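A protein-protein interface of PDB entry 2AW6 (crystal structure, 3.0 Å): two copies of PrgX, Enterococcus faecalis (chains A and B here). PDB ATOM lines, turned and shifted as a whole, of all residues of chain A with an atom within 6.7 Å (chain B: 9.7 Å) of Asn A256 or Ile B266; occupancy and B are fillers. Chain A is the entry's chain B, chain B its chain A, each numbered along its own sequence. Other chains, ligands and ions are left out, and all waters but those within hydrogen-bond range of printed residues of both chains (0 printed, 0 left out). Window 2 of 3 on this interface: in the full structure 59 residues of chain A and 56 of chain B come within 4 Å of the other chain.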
ATOM      1  N   ASN A 237      30.137 -26.354   0.981  1.00  0.00           N
ATOM      2  CA  ASN A 237      29.264 -25.920   2.052  1.00  0.00           C
ATOM      3  C   ASN A 237      28.414 -27.049   2.632  1.00  0.00           C
ATOM      4  O   ASN A 237      28.201 -27.108   3.846  1.00  0.00           O
ATOM      5  CB  ASN A 237      28.390 -24.770   1.599  1.00  0.00           C
ATOM      6  CG  ASN A 237      29.041 -23.434   1.832  1.00  0.00           C
ATOM      7  OD1 ASN A 237      29.102 -22.950   2.961  1.00  0.00           O
ATOM      8  ND2 ASN A 237      29.533 -22.823   0.762  1.00  0.00           N
ATOM      9  N   TYR A 238      27.940 -27.956   1.783  1.00  0.00           N
ATOM     10  CA  TYR A 238      27.264 -29.151   2.279  1.00  0.00           C
ATOM     11  C   TYR A 238      28.205 -29.987   3.160  1.00  0.00           C
ATOM     12  O   TYR A 238      27.806 -30.460   4.225  1.00  0.00           O
ATOM     13  CB  TYR A 238      26.665 -29.958   1.124  1.00  0.00           C
ATOM     14  CG  TYR A 238      27.059 -31.413   1.126  1.00  0.00           C
ATOM     15  CD1 TYR A 238      28.060 -31.875   0.278  1.00  0.00           C
ATOM     16  CD2 TYR A 238      26.450 -32.322   1.983  1.00  0.00           C
ATOM     17  CE1 TYR A 238      28.444 -33.195   0.279  1.00  0.00           C
ATOM     18  CE2 TYR A 238      26.828 -33.652   1.990  1.00  0.00           C
ATOM     19  CZ  TYR A 238      27.823 -34.082   1.131  1.00  0.00           C
ATOM     20  OH  TYR A 238      28.200 -35.401   1.126  1.00  0.00           O
ATOM     21  N   LYS A 240      30.898 -28.763   4.680  1.00  0.00           N
ATOM     22  CA  LYS A 240      31.135 -27.895   5.831  1.00  0.00           C
ATOM     23  C   LYS A 240      29.980 -28.084   6.804  1.00  0.00           C
ATOM     24  O   LYS A 240      30.176 -28.195   8.019  1.00  0.00           O
ATOM     25  CB  LYS A 240      31.285 -26.423   5.374  1.00  0.00           C
ATOM     26  CG  LYS A 240      30.728 -25.345   6.311  1.00  0.00           C
ATOM     27  CD  LYS A 240      31.796 -24.607   7.106  1.00  0.00           C
ATOM     28  CE  LYS A 240      32.353 -23.404   6.345  1.00  0.00           C
ATOM     29  NZ  LYS A 240      31.373 -22.745   5.435  1.00  0.00           N
ATOM     30  N   GLN A 241      28.779 -28.151   6.239  1.00  0.00           N
ATOM     31  CA  GLN A 241      27.567 -28.275   7.019  1.00  0.00           C
ATOM     32  C   GLN A 241      27.525 -29.619   7.739  1.00  0.00           C
ATOM     33  O   GLN A 241      27.107 -29.686   8.896  1.00  0.00           O
ATOM     34  CB  GLN A 241      26.340 -28.057   6.138  1.00  0.00           C
ATOM     35  CG  GLN A 241      25.199 -27.346   6.844  1.00  0.00           C
ATOM     36  CD  GLN A 241      25.509 -25.910   7.255  1.00  0.00           C
ATOM     37  OE1 GLN A 241      25.322 -25.538   8.412  1.00  0.00           O
ATOM     38  NE2 GLN A 241      25.971 -25.100   6.309  1.00  0.00           N
ATOM     39  N   GLN A 244      30.003 -29.526  10.718  1.00  0.00           N
ATOM     40  CA  GLN A 244      29.365 -28.892  11.878  1.00  0.00           C
ATOM     41  C   GLN A 244      28.356 -29.820  12.559  1.00  0.00           C
ATOM     42  O   GLN A 244      28.037 -29.640  13.736  1.00  0.00           O
ATOM     43  CB  GLN A 244      28.669 -27.586  11.475  1.00  0.00           C
ATOM     44  CG  GLN A 244      29.598 -26.478  10.945  1.00  0.00           C
ATOM     45  CD  GLN A 244      28.850 -25.229  10.461  1.00  0.00           C
ATOM     46  OE1 GLN A 244      27.685 -24.997  10.801  1.00  0.00           O
ATOM     47  NE2 GLN A 244      29.530 -24.419   9.662  1.00  0.00           N
ATOM     48  N   ASN A 250      24.583 -30.830  16.529  1.00  0.00           N
ATOM     49  CA  ASN A 250      23.360 -30.067  16.314  1.00  0.00           C
ATOM     50  C   ASN A 250      22.702 -30.446  14.990  1.00  0.00           C
ATOM     51  O   ASN A 250      23.335 -30.399  13.937  1.00  0.00           O
ATOM     52  CB  ASN A 250      23.672 -28.567  16.344  1.00  0.00           C
ATOM     53  CG  ASN A 250      22.707 -27.747  15.501  1.00  0.00           C
ATOM     54  OD1 ASN A 250      21.585 -27.453  15.917  1.00  0.00           O
ATOM     55  ND2 ASN A 250      23.146 -27.375  14.305  1.00  0.00           N
ATOM     56  N   ILE A 251      21.419 -30.784  15.058  1.00  0.00           N
ATOM     57  CA  ILE A 251      20.688 -31.376  13.937  1.00  0.00           C
ATOM     58  C   ILE A 251      20.371 -30.386  12.803  1.00  0.00           C
ATOM     59  O   ILE A 251      20.211 -30.792  11.652  1.00  0.00           O
ATOM     60  CB  ILE A 251      19.416 -32.118  14.451  1.00  0.00           C
ATOM     61  CG1 ILE A 251      18.527 -32.613  13.302  1.00  0.00           C
ATOM     62  CG2 ILE A 251      18.641 -31.247  15.442  1.00  0.00           C
ATOM     63  CD1 ILE A 251      19.000 -33.893  12.645  1.00  0.00           C
ATOM     64  N   ASP A 252      20.303 -29.094  13.126  1.00  0.00           N
ATOM     65  CA  ASP A 252      20.044 -28.055  12.119  1.00  0.00           C
ATOM     66  C   ASP A 252      21.037 -28.128  10.963  1.00  0.00           C
ATOM     67  O   ASP A 252      20.653 -27.994   9.802  1.00  0.00           O
ATOM     68  CB  ASP A 252      20.080 -26.655  12.742  1.00  0.00           C
ATOM     69  CG  ASP A 252      18.867 -26.367  13.603  1.00  0.00           C
ATOM     70  OD1 ASP A 252      17.772 -26.891  13.300  1.00  0.00           O
ATOM     71  OD2 ASP A 252      19.008 -25.608  14.584  1.00  0.00           O
ATOM     72  N   SER A 253      22.310 -28.343  11.293  1.00  0.00           N
ATOM     73  CA  SER A 253      23.376 -28.459  10.299  1.00  0.00           C
ATOM     74  C   SER A 253      23.100 -29.584   9.310  1.00  0.00           C
ATOM     75  O   SER A 253      23.257 -29.409   8.105  1.00  0.00           O
ATOM     76  CB  SER A 253      24.729 -28.686  10.981  1.00  0.00           C
ATOM     77  OG  SER A 253      25.232 -27.496  11.566  1.00  0.00           O
ATOM     78  N   TYR A 254      22.685 -30.738   9.823  1.00  0.00           N
ATOM     79  CA  TYR A 254      22.322 -31.857   8.962  1.00  0.00           C
ATOM     80  C   TYR A 254      21.279 -31.445   7.914  1.00  0.00           C
ATOM     81  O   TYR A 254      21.452 -31.704   6.720  1.00  0.00           O
ATOM     82  CB  TYR A 254      21.799 -33.043   9.783  1.00  0.00           C
ATOM     83  CG  TYR A 254      21.330 -34.189   8.918  1.00  0.00           C
ATOM     84  CD1 TYR A 254      19.989 -34.314   8.551  1.00  0.00           C
ATOM     85  CD2 TYR A 254      22.233 -35.129   8.441  1.00  0.00           C
ATOM     86  CE1 TYR A 254      19.559 -35.365   7.743  1.00  0.00           C
ATOM     87  CE2 TYR A 254      21.822 -36.180   7.631  1.00  0.00           C
ATOM     88  CZ  TYR A 254      20.484 -36.297   7.283  1.00  0.00           C
ATOM     89  OH  TYR A 254      20.091 -37.347   6.475  1.00  0.00           O
ATOM     90  N   LEU A 255      20.201 -30.815   8.388  1.00  0.00           N
ATOM     91  CA  LEU A 255      19.112 -30.310   7.538  1.00  0.00           C
ATOM     92  C   LEU A 255      19.628 -29.400   6.450  1.00  0.00           C
ATOM     93  O   LEU A 255      19.240 -29.531   5.286  1.00  0.00           O
ATOM     94  CB  LEU A 255      18.089 -29.519   8.366  1.00  0.00           C
ATOM     95  CG  LEU A 255      16.863 -30.198   8.981  1.00  0.00           C
ATOM     96  CD1 LEU A 255      16.077 -30.982   7.936  1.00  0.00           C
ATOM     97  CD2 LEU A 255      17.256 -31.089  10.146  1.00  0.00           C
ATOM     98  N   ASN A 256      20.482 -28.458   6.850  1.00  0.00           N
ATOM     99  CA  ASN A 256      21.130 -27.564   5.908  1.00  0.00           C
ATOM    100  C   ASN A 256      21.810 -28.389   4.823  1.00  0.00           C
ATOM    101  O   ASN A 256      21.525 -28.229   3.638  1.00  0.00           O
ATOM    102  CB  ASN A 256      22.160 -26.661   6.603  1.00  0.00           C
ATOM    103  CG  ASN A 256      21.534 -25.517   7.376  1.00  0.00           C
ATOM    104  OD1 ASN A 256      20.462 -25.026   7.035  1.00  0.00           O
ATOM    105  ND2 ASN A 256      22.221 -25.069   8.414  1.00  0.00           N
ATOM    106  N   ALA A 257      22.688 -29.293   5.237  1.00  0.00           N
ATOM    107  CA  ALA A 257      23.385 -30.143   4.283  1.00  0.00           C
ATOM    108  C   ALA A 257      22.399 -30.773   3.305  1.00  0.00           C
ATOM    109  O   ALA A 257      22.609 -30.722   2.099  1.00  0.00           O
ATOM    110  CB  ALA A 257      24.213 -31.200   4.996  1.00  0.00           C
ATOM    111  N   VAL A 258      21.308 -31.331   3.826  1.00  0.00           N
ATOM    112  CA  VAL A 258      20.306 -31.975   2.980  1.00  0.00           C
ATOM    113  C   VAL A 258      19.724 -30.936   2.038  1.00  0.00           C
ATOM    114  O   VAL A 258      19.757 -31.108   0.824  1.00  0.00           O
ATOM    115  CB  VAL A 258      19.196 -32.676   3.803  1.00  0.00           C
ATOM    116  CG1 VAL A 258      18.134 -33.269   2.879  1.00  0.00           C
ATOM    117  CG2 VAL A 258      19.793 -33.757   4.677  1.00  0.00           C
ATOM    118  N   ASN A 259      19.246 -29.838   2.612  1.00  0.00           N
ATOM    119  CA  ASN A 259      18.677 -28.729   1.862  1.00  0.00           C
ATOM    120  C   ASN A 259      19.556 -28.234   0.695  1.00  0.00           C
ATOM    121  O   ASN A 259      19.040 -27.848  -0.350  1.00  0.00           O
ATOM    122  CB  ASN A 259      18.368 -27.590   2.832  1.00  0.00           C
ATOM    123  CG  ASN A 259      17.296 -26.673   2.327  1.00  0.00           C
ATOM    124  OD1 ASN A 259      16.495 -27.047   1.466  1.00  0.00           O
ATOM    125  ND2 ASN A 259      17.266 -25.454   2.859  1.00  0.00           N
ATOM    126  N   ILE A 260      20.877 -28.263   0.891  1.00  0.00           N
ATOM    127  CA  ILE A 260      21.859 -27.892  -0.135  1.00  0.00           C
ATOM    128  C   ILE A 260      21.860 -28.928  -1.260  1.00  0.00           C
ATOM    129  O   ILE A 260      21.781 -28.576  -2.444  1.00  0.00           O
ATOM    130  CB  ILE A 260      23.299 -27.755   0.463  1.00  0.00           C
ATOM    131  CG1 ILE A 260      23.350 -26.618   1.487  1.00  0.00           C
ATOM    132  CG2 ILE A 260      24.319 -27.477  -0.619  1.00  0.00           C
ATOM    133  CD1 ILE A 260      24.610 -26.573   2.336  1.00  0.00           C
ATOM    134  N   ILE A 261      21.939 -30.199  -0.870  1.00  0.00           N
ATOM    135  CA  ILE A 261      21.990 -31.313  -1.805  1.00  0.00           C
ATOM    136  C   ILE A 261      20.776 -31.301  -2.709  1.00  0.00           C
ATOM    137  O   ILE A 261      20.899 -31.415  -3.927  1.00  0.00           O
ATOM    138  CB  ILE A 261      22.046 -32.664  -1.071  1.00  0.00           C
ATOM    139  CG1 ILE A 261      23.356 -32.789  -0.288  1.00  0.00           C
ATOM    140  CG2 ILE A 261      21.894 -33.813  -2.063  1.00  0.00           C
ATOM    141  CD1 ILE A 261      23.428 -33.993   0.615  1.00  0.00           C
ATOM    142  N   LEU B 234      21.814 -20.968 -10.408  1.00  0.00           N
ATOM    143  CA  LEU B 234      20.922 -20.863  -9.255  1.00  0.00           C
ATOM    144  C   LEU B 234      19.947 -19.711  -9.390  1.00  0.00           C
ATOM    145  O   LEU B 234      18.767 -19.869  -9.131  1.00  0.00           O
ATOM    146  CB  LEU B 234      21.722 -20.667  -7.974  1.00  0.00           C
ATOM    147  CG  LEU B 234      22.437 -21.846  -7.333  1.00  0.00           C
ATOM    148  CD1 LEU B 234      23.179 -21.372  -6.091  1.00  0.00           C
ATOM    149  CD2 LEU B 234      21.436 -22.925  -6.961  1.00  0.00           C
ATOM    150  N   VAL B 258      11.894 -19.740  -3.227  1.00  0.00           N
ATOM    151  CA  VAL B 258      12.337 -19.263  -1.926  1.00  0.00           C
ATOM    152  C   VAL B 258      13.513 -20.108  -1.450  1.00  0.00           C
ATOM    153  O   VAL B 258      14.561 -19.571  -1.072  1.00  0.00           O
ATOM    154  CB  VAL B 258      11.180 -19.269  -0.892  1.00  0.00           C
ATOM    155  CG1 VAL B 258      11.699 -19.142   0.533  1.00  0.00           C
ATOM    156  CG2 VAL B 258      10.209 -18.140  -1.186  1.00  0.00           C
ATOM    157  N   ASN B 259      13.346 -21.427  -1.501  1.00  0.00           N
ATOM    158  CA  ASN B 259      14.381 -22.356  -1.051  1.00  0.00           C
ATOM    159  C   ASN B 259      15.716 -22.183  -1.774  1.00  0.00           C
ATOM    160  O   ASN B 259      16.775 -22.366  -1.162  1.00  0.00           O
ATOM    161  CB  ASN B 259      13.888 -23.803  -1.122  1.00  0.00           C
ATOM    162  CG  ASN B 259      12.722 -24.064  -0.183  1.00  0.00           C
ATOM    163  OD1 ASN B 259      12.645 -23.490   0.906  1.00  0.00           O
ATOM    164  ND2 ASN B 259      11.803 -24.925  -0.604  1.00  0.00           N
ATOM    165  N   ILE B 260      15.660 -21.816  -3.058  1.00  0.00           N
ATOM    166  CA  ILE B 260      16.861 -21.485  -3.838  1.00  0.00           C
ATOM    167  C   ILE B 260      17.539 -20.232  -3.284  1.00  0.00           C
ATOM    168  O   ILE B 260      18.740 -20.238  -3.014  1.00  0.00           O
ATOM    169  CB  ILE B 260      16.556 -21.265  -5.349  1.00  0.00           C
ATOM    170  CG1 ILE B 260      16.040 -22.550  -6.002  1.00  0.00           C
ATOM    171  CG2 ILE B 260      17.799 -20.754  -6.085  1.00  0.00           C
ATOM    172  CD1 ILE B 260      15.546 -22.379  -7.437  1.00  0.00           C
ATOM    173  N   ILE B 261      16.758 -19.167  -3.116  1.00  0.00           N
ATOM    174  CA  ILE B 261      17.259 -17.890  -2.622  1.00  0.00           C
ATOM    175  C   ILE B 261      17.934 -18.071  -1.282  1.00  0.00           C
ATOM    176  O   ILE B 261      19.054 -17.611  -1.085  1.00  0.00           O
ATOM    177  CB  ILE B 261      16.132 -16.835  -2.505  1.00  0.00           C
ATOM    178  CG1 ILE B 261      15.627 -16.444  -3.895  1.00  0.00           C
ATOM    179  CG2 ILE B 261      16.612 -15.586  -1.725  1.00  0.00           C
ATOM    180  CD1 ILE B 261      14.453 -15.507  -3.880  1.00  0.00           C
ATOM    181  N   ASN B 262      17.251 -18.757  -0.370  1.00  0.00           N
ATOM    182  CA  ASN B 262      17.815 -19.072   0.940  1.00  0.00           C
ATOM    183  C   ASN B 262      19.204 -19.690   0.844  1.00  0.00           C
ATOM    184  O   ASN B 262      20.099 -19.341   1.616  1.00  0.00           O
ATOM    185  CB  ASN B 262      16.903 -20.029   1.713  1.00  0.00           C
ATOM    186  CG  ASN B 262      15.580 -19.404   2.082  1.00  0.00           C
ATOM    187  OD1 ASN B 262      15.525 -18.291   2.608  1.00  0.00           O
ATOM    188  ND2 ASN B 262      14.500 -20.126   1.820  1.00  0.00           N
ATOM    189  N   ILE B 263      19.384 -20.602  -0.110  1.00  0.00           N
ATOM    190  CA  ILE B 263      20.645 -21.336  -0.222  1.00  0.00           C
ATOM    191  C   ILE B 263      21.811 -20.364  -0.385  1.00  0.00           C
ATOM    192  O   ILE B 263      22.909 -20.629   0.108  1.00  0.00           O
ATOM    193  CB  ILE B 263      20.601 -22.460  -1.316  1.00  0.00           C
ATOM    194  CG1 ILE B 263      20.781 -23.841  -0.671  1.00  0.00           C
ATOM    195  CG2 ILE B 263      21.645 -22.242  -2.394  1.00  0.00           C
ATOM    196  CD1 ILE B 263      19.682 -24.223   0.317  1.00  0.00           C
ATOM    197  N   PHE B 264      21.540 -19.225  -1.033  1.00  0.00           N
ATOM    198  CA  PHE B 264      22.505 -18.129  -1.132  1.00  0.00           C
ATOM    199  C   PHE B 264      22.970 -17.648   0.236  1.00  0.00           C
ATOM    200  O   PHE B 264      24.165 -17.456   0.422  1.00  0.00           O
ATOM    201  CB  PHE B 264      21.961 -16.967  -1.956  1.00  0.00           C
ATOM    202  CG  PHE B 264      22.093 -17.158  -3.441  1.00  0.00           C
ATOM    203  CD1 PHE B 264      23.240 -16.745  -4.114  1.00  0.00           C
ATOM    204  CD2 PHE B 264      21.071 -17.741  -4.180  1.00  0.00           C
ATOM    205  CE1 PHE B 264      23.361 -16.913  -5.509  1.00  0.00           C
ATOM    206  CE2 PHE B 264      21.192 -17.909  -5.575  1.00  0.00           C
ATOM    207  CZ  PHE B 264      22.335 -17.493  -6.233  1.00  0.00           C
ATOM    208  N   LYS B 265      22.045 -17.468   1.183  1.00  0.00           N
ATOM    209  CA  LYS B 265      22.400 -17.139   2.575  1.00  0.00           C
ATOM    210  C   LYS B 265      23.243 -18.244   3.210  1.00  0.00           C
ATOM    211  O   LYS B 265      24.321 -17.989   3.759  1.00  0.00           O
ATOM    212  CB  LYS B 265      21.143 -16.923   3.421  1.00  0.00           C
ATOM    213  CG  LYS B 265      21.397 -16.406   4.836  1.00  0.00           C
ATOM    214  CD  LYS B 265      20.088 -16.001   5.500  1.00  0.00           C
ATOM    215  CE  LYS B 265      20.307 -15.046   6.660  1.00  0.00           C
ATOM    216  NZ  LYS B 265      20.886 -15.730   7.848  1.00  0.00           N
ATOM    217  N   ILE B 266      22.742 -19.470   3.117  1.00  0.00           N
ATOM    218  CA  ILE B 266      23.384 -20.633   3.711  1.00  0.00           C
ATOM    219  C   ILE B 266      24.834 -20.834   3.232  1.00  0.00           C
ATOM    220  O   ILE B 266      25.629 -21.478   3.917  1.00  0.00           O
ATOM    221  CB  ILE B 266      22.524 -21.911   3.478  1.00  0.00           C
ATOM    222  CG1 ILE B 266      21.447 -22.055   4.563  1.00  0.00           C
ATOM    223  CG2 ILE B 266      23.385 -23.158   3.463  1.00  0.00           C
ATOM    224  CD1 ILE B 266      20.035 -21.732   4.101  1.00  0.00           C
ATOM    225  N   ILE B 267      25.177 -20.290   2.064  1.00  0.00           N
ATOM    226  CA  ILE B 267      26.553 -20.388   1.543  1.00  0.00           C
ATOM    227  C   ILE B 267      27.301 -19.057   1.575  1.00  0.00           C
ATOM    228  O   ILE B 267      28.319 -18.883   0.897  1.00  0.00           O
ATOM    229  CB  ILE B 267      26.639 -21.039   0.130  1.00  0.00           C
ATOM    230  CG1 ILE B 267      25.991 -20.138  -0.936  1.00  0.00           C
ATOM    231  CG2 ILE B 267      26.054 -22.445   0.167  1.00  0.00           C
ATOM    232  CD1 ILE B 267      26.138 -20.635  -2.347  1.00  0.00           C
ATOM    233  N   GLY B 268      26.777 -18.126   2.363  1.00  0.00           N
ATOM    234  CA  GLY B 268      27.487 -16.900   2.690  1.00  0.00           C
ATOM    235  C   GLY B 268      27.497 -15.792   1.657  1.00  0.00           C
ATOM    236  O   GLY B 268      28.235 -14.823   1.812  1.00  0.00           O
ATOM    237  N   LYS B 269      26.690 -15.910   0.605  1.00  0.00           N
ATOM    238  CA  LYS B 269      26.576 -14.823  -0.371  1.00  0.00           C
ATOM    239  C   LYS B 269      25.563 -13.811   0.150  1.00  0.00           C
ATOM    240  O   LYS B 269      24.501 -13.597  -0.437  1.00  0.00           O
ATOM    241  CB  LYS B 269      26.230 -15.342  -1.776  1.00  0.00           C
ATOM    242  CG  LYS B 269      27.159 -16.457  -2.341  1.00  0.00           C
ATOM    243  CD  LYS B 269      28.666 -16.157  -2.249  1.00  0.00           C
ATOM    244  CE  LYS B 269      29.090 -14.981  -3.121  1.00  0.00           C
ATOM    245  NZ  LYS B 269      29.109 -15.295  -4.574  1.00  0.00           N
ATOM    246  N   GLU B 270      25.938 -13.188   1.264  1.00  0.00           N
ATOM    247  CA  GLU B 270      25.050 -12.380   2.090  1.00  0.00           C
ATOM    248  C   GLU B 270      24.334 -11.280   1.318  1.00  0.00           C
ATOM    249  O   GLU B 270      23.106 -11.224   1.310  1.00  0.00           O
ATOM    250  CB  GLU B 270      25.827 -11.808   3.286  1.00  0.00           C
ATOM    251  CG  GLU B 270      24.960 -11.352   4.463  1.00  0.00           C
ATOM    252  CD  GLU B 270      24.114 -12.471   5.063  1.00  0.00           C
ATOM    253  OE1 GLU B 270      24.541 -13.646   5.038  1.00  0.00           O
ATOM    254  OE2 GLU B 270      23.015 -12.171   5.569  1.00  0.00           O
ATOM    255  N   ASP B 271      25.103 -10.416   0.664  1.00  0.00           N
ATOM    256  CA  ASP B 271      24.536  -9.286  -0.076  1.00  0.00           C
ATOM    257  C   ASP B 271      23.722  -9.699  -1.313  1.00  0.00           C
ATOM    258  O   ASP B 271      22.743  -9.029  -1.662  1.00  0.00           O
ATOM    259  CB  ASP B 271      25.610  -8.246  -0.427  1.00  0.00           C
ATOM    260  CG  ASP B 271      26.944  -8.871  -0.803  1.00  0.00           C
ATOM    261  OD1 ASP B 271      27.889  -8.096  -1.058  1.00  0.00           O
ATOM    262  OD2 ASP B 271      27.058 -10.120  -0.843  1.00  0.00           O
ATOM    263  N   ILE B 272      24.112 -10.797  -1.962  1.00  0.00           N
ATOM    264  CA  ILE B 272      23.347 -11.316  -3.103  1.00  0.00           C
ATOM    265  C   ILE B 272      22.007 -11.857  -2.613  1.00  0.00           C
ATOM    266  O   ILE B 272      20.987 -11.645  -3.270  1.00  0.00           O
ATOM    267  CB  ILE B 272      24.156 -12.345  -3.974  1.00  0.00           C
ATOM    268  CG1 ILE B 272      25.083 -11.601  -4.947  1.00  0.00           C
ATOM    269  CG2 ILE B 272      23.229 -13.268  -4.784  1.00  0.00           C
ATOM    270  CD1 ILE B 272      26.410 -12.304  -5.231  1.00  0.00           C
ATOM    271  N   HIS B 273      22.014 -12.515  -1.451  1.00  0.00           N
ATOM    272  CA  HIS B 273      20.784 -12.997  -0.813  1.00  0.00           C
ATOM    273  C   HIS B 273      19.822 -11.851  -0.490  1.00  0.00           C
ATOM    274  O   HIS B 273      18.621 -11.962  -0.749  1.00  0.00           O
ATOM    275  CB  HIS B 273      21.100 -13.796   0.449  1.00  0.00           C
ATOM    276  CG  HIS B 273      19.886 -14.273   1.187  1.00  0.00           C
ATOM    277  ND1 HIS B 273      19.255 -13.517   2.152  1.00  0.00           N
ATOM    278  CD2 HIS B 273      19.192 -15.434   1.108  1.00  0.00           C
ATOM    279  CE1 HIS B 273      18.225 -14.191   2.635  1.00  0.00           C
ATOM    280  NE2 HIS B 273      18.166 -15.358   2.019  1.00  0.00           N
ATOM    281  N   ARG B 274      20.353 -10.759   0.072  1.00  0.00           N
ATOM    282  CA  ARG B 274      19.577  -9.538   0.340  1.00  0.00           C
ATOM    283  C   ARG B 274      18.939  -8.987  -0.939  1.00  0.00           C
ATOM    284  O   ARG B 274      17.722  -8.791  -1.000  1.00  0.00           O
ATOM    285  CB  ARG B 274      20.445  -8.471   1.017  1.00  0.00           C
ATOM    286  CG  ARG B 274      20.446  -8.534   2.543  1.00  0.00           C
ATOM    287  CD  ARG B 274      21.766  -8.040   3.124  1.00  0.00           C
ATOM    288  NE  ARG B 274      22.151  -6.732   2.594  1.00  0.00           N
ATOM    289  CZ  ARG B 274      23.407  -6.310   2.455  1.00  0.00           C
ATOM    290  NH1 ARG B 274      24.425  -7.091   2.797  1.00  0.00           N
ATOM    291  NH2 ARG B 274      23.646  -5.102   1.962  1.00  0.00           N
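OD1 of Asn A237 touches O of Ile B266 (3.9 Å). Asn A237 touches Ile B267 (ND2 to CB, 3.5 Å). Asn A256 touches Ile B266 (OD1 to CG1, 3.99 Å). Ile B263 touches Asn A259. Ile B266 touches Ile A260.
Hydrophobic or aromatic side chains of chain A that line the printed part of chain B: Ile A260. Hydrophobic or aromatic side chains of chain B within 4 Å of the printed part of chain A: Ile B263, Ile B266 and Ile B267. Along chain B the printed residues that touch a printed residue of chain A span positions 263 to 267. Among the printed residues, no Asp or Glu carboxylate lies within 4 Å of a Lys or Arg side-chain nitrogen of the other chain.
Of the printed residues of chain B, Asn A256 touches Ile B266 (3.99 Å). Printed residues of chain A within 4 Å of Ile B266: Asn A237 (3.9 Å), Asn A256 (3.99 Å) and Ile A260 (3.8 Å). No residue of chain B comes within 4 Å of Ser A253. No residue of chain B comes within 4 Å of Ala A257. Of the printed residues of chain B, Asn A237 touches Ile B266 (3.9 Å) and Ile B267 (3.5 Å). Of the printed residues of chain B, Ile A260 touches Ile B266.
Positions printed for both chains: 258, 259, 260 and 261. Of the 5 pairs that touch across the chains among the printed residues, none has its exchanged pair printed and touching as well.
OD1 of Asn A237 lies within hydrogen-bond range of NZ of Lys A240 (3.4 Å). ND2 of Asn A256 is in hydrogen-bond range of OE1 of Gln A241 (3.1 Å).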
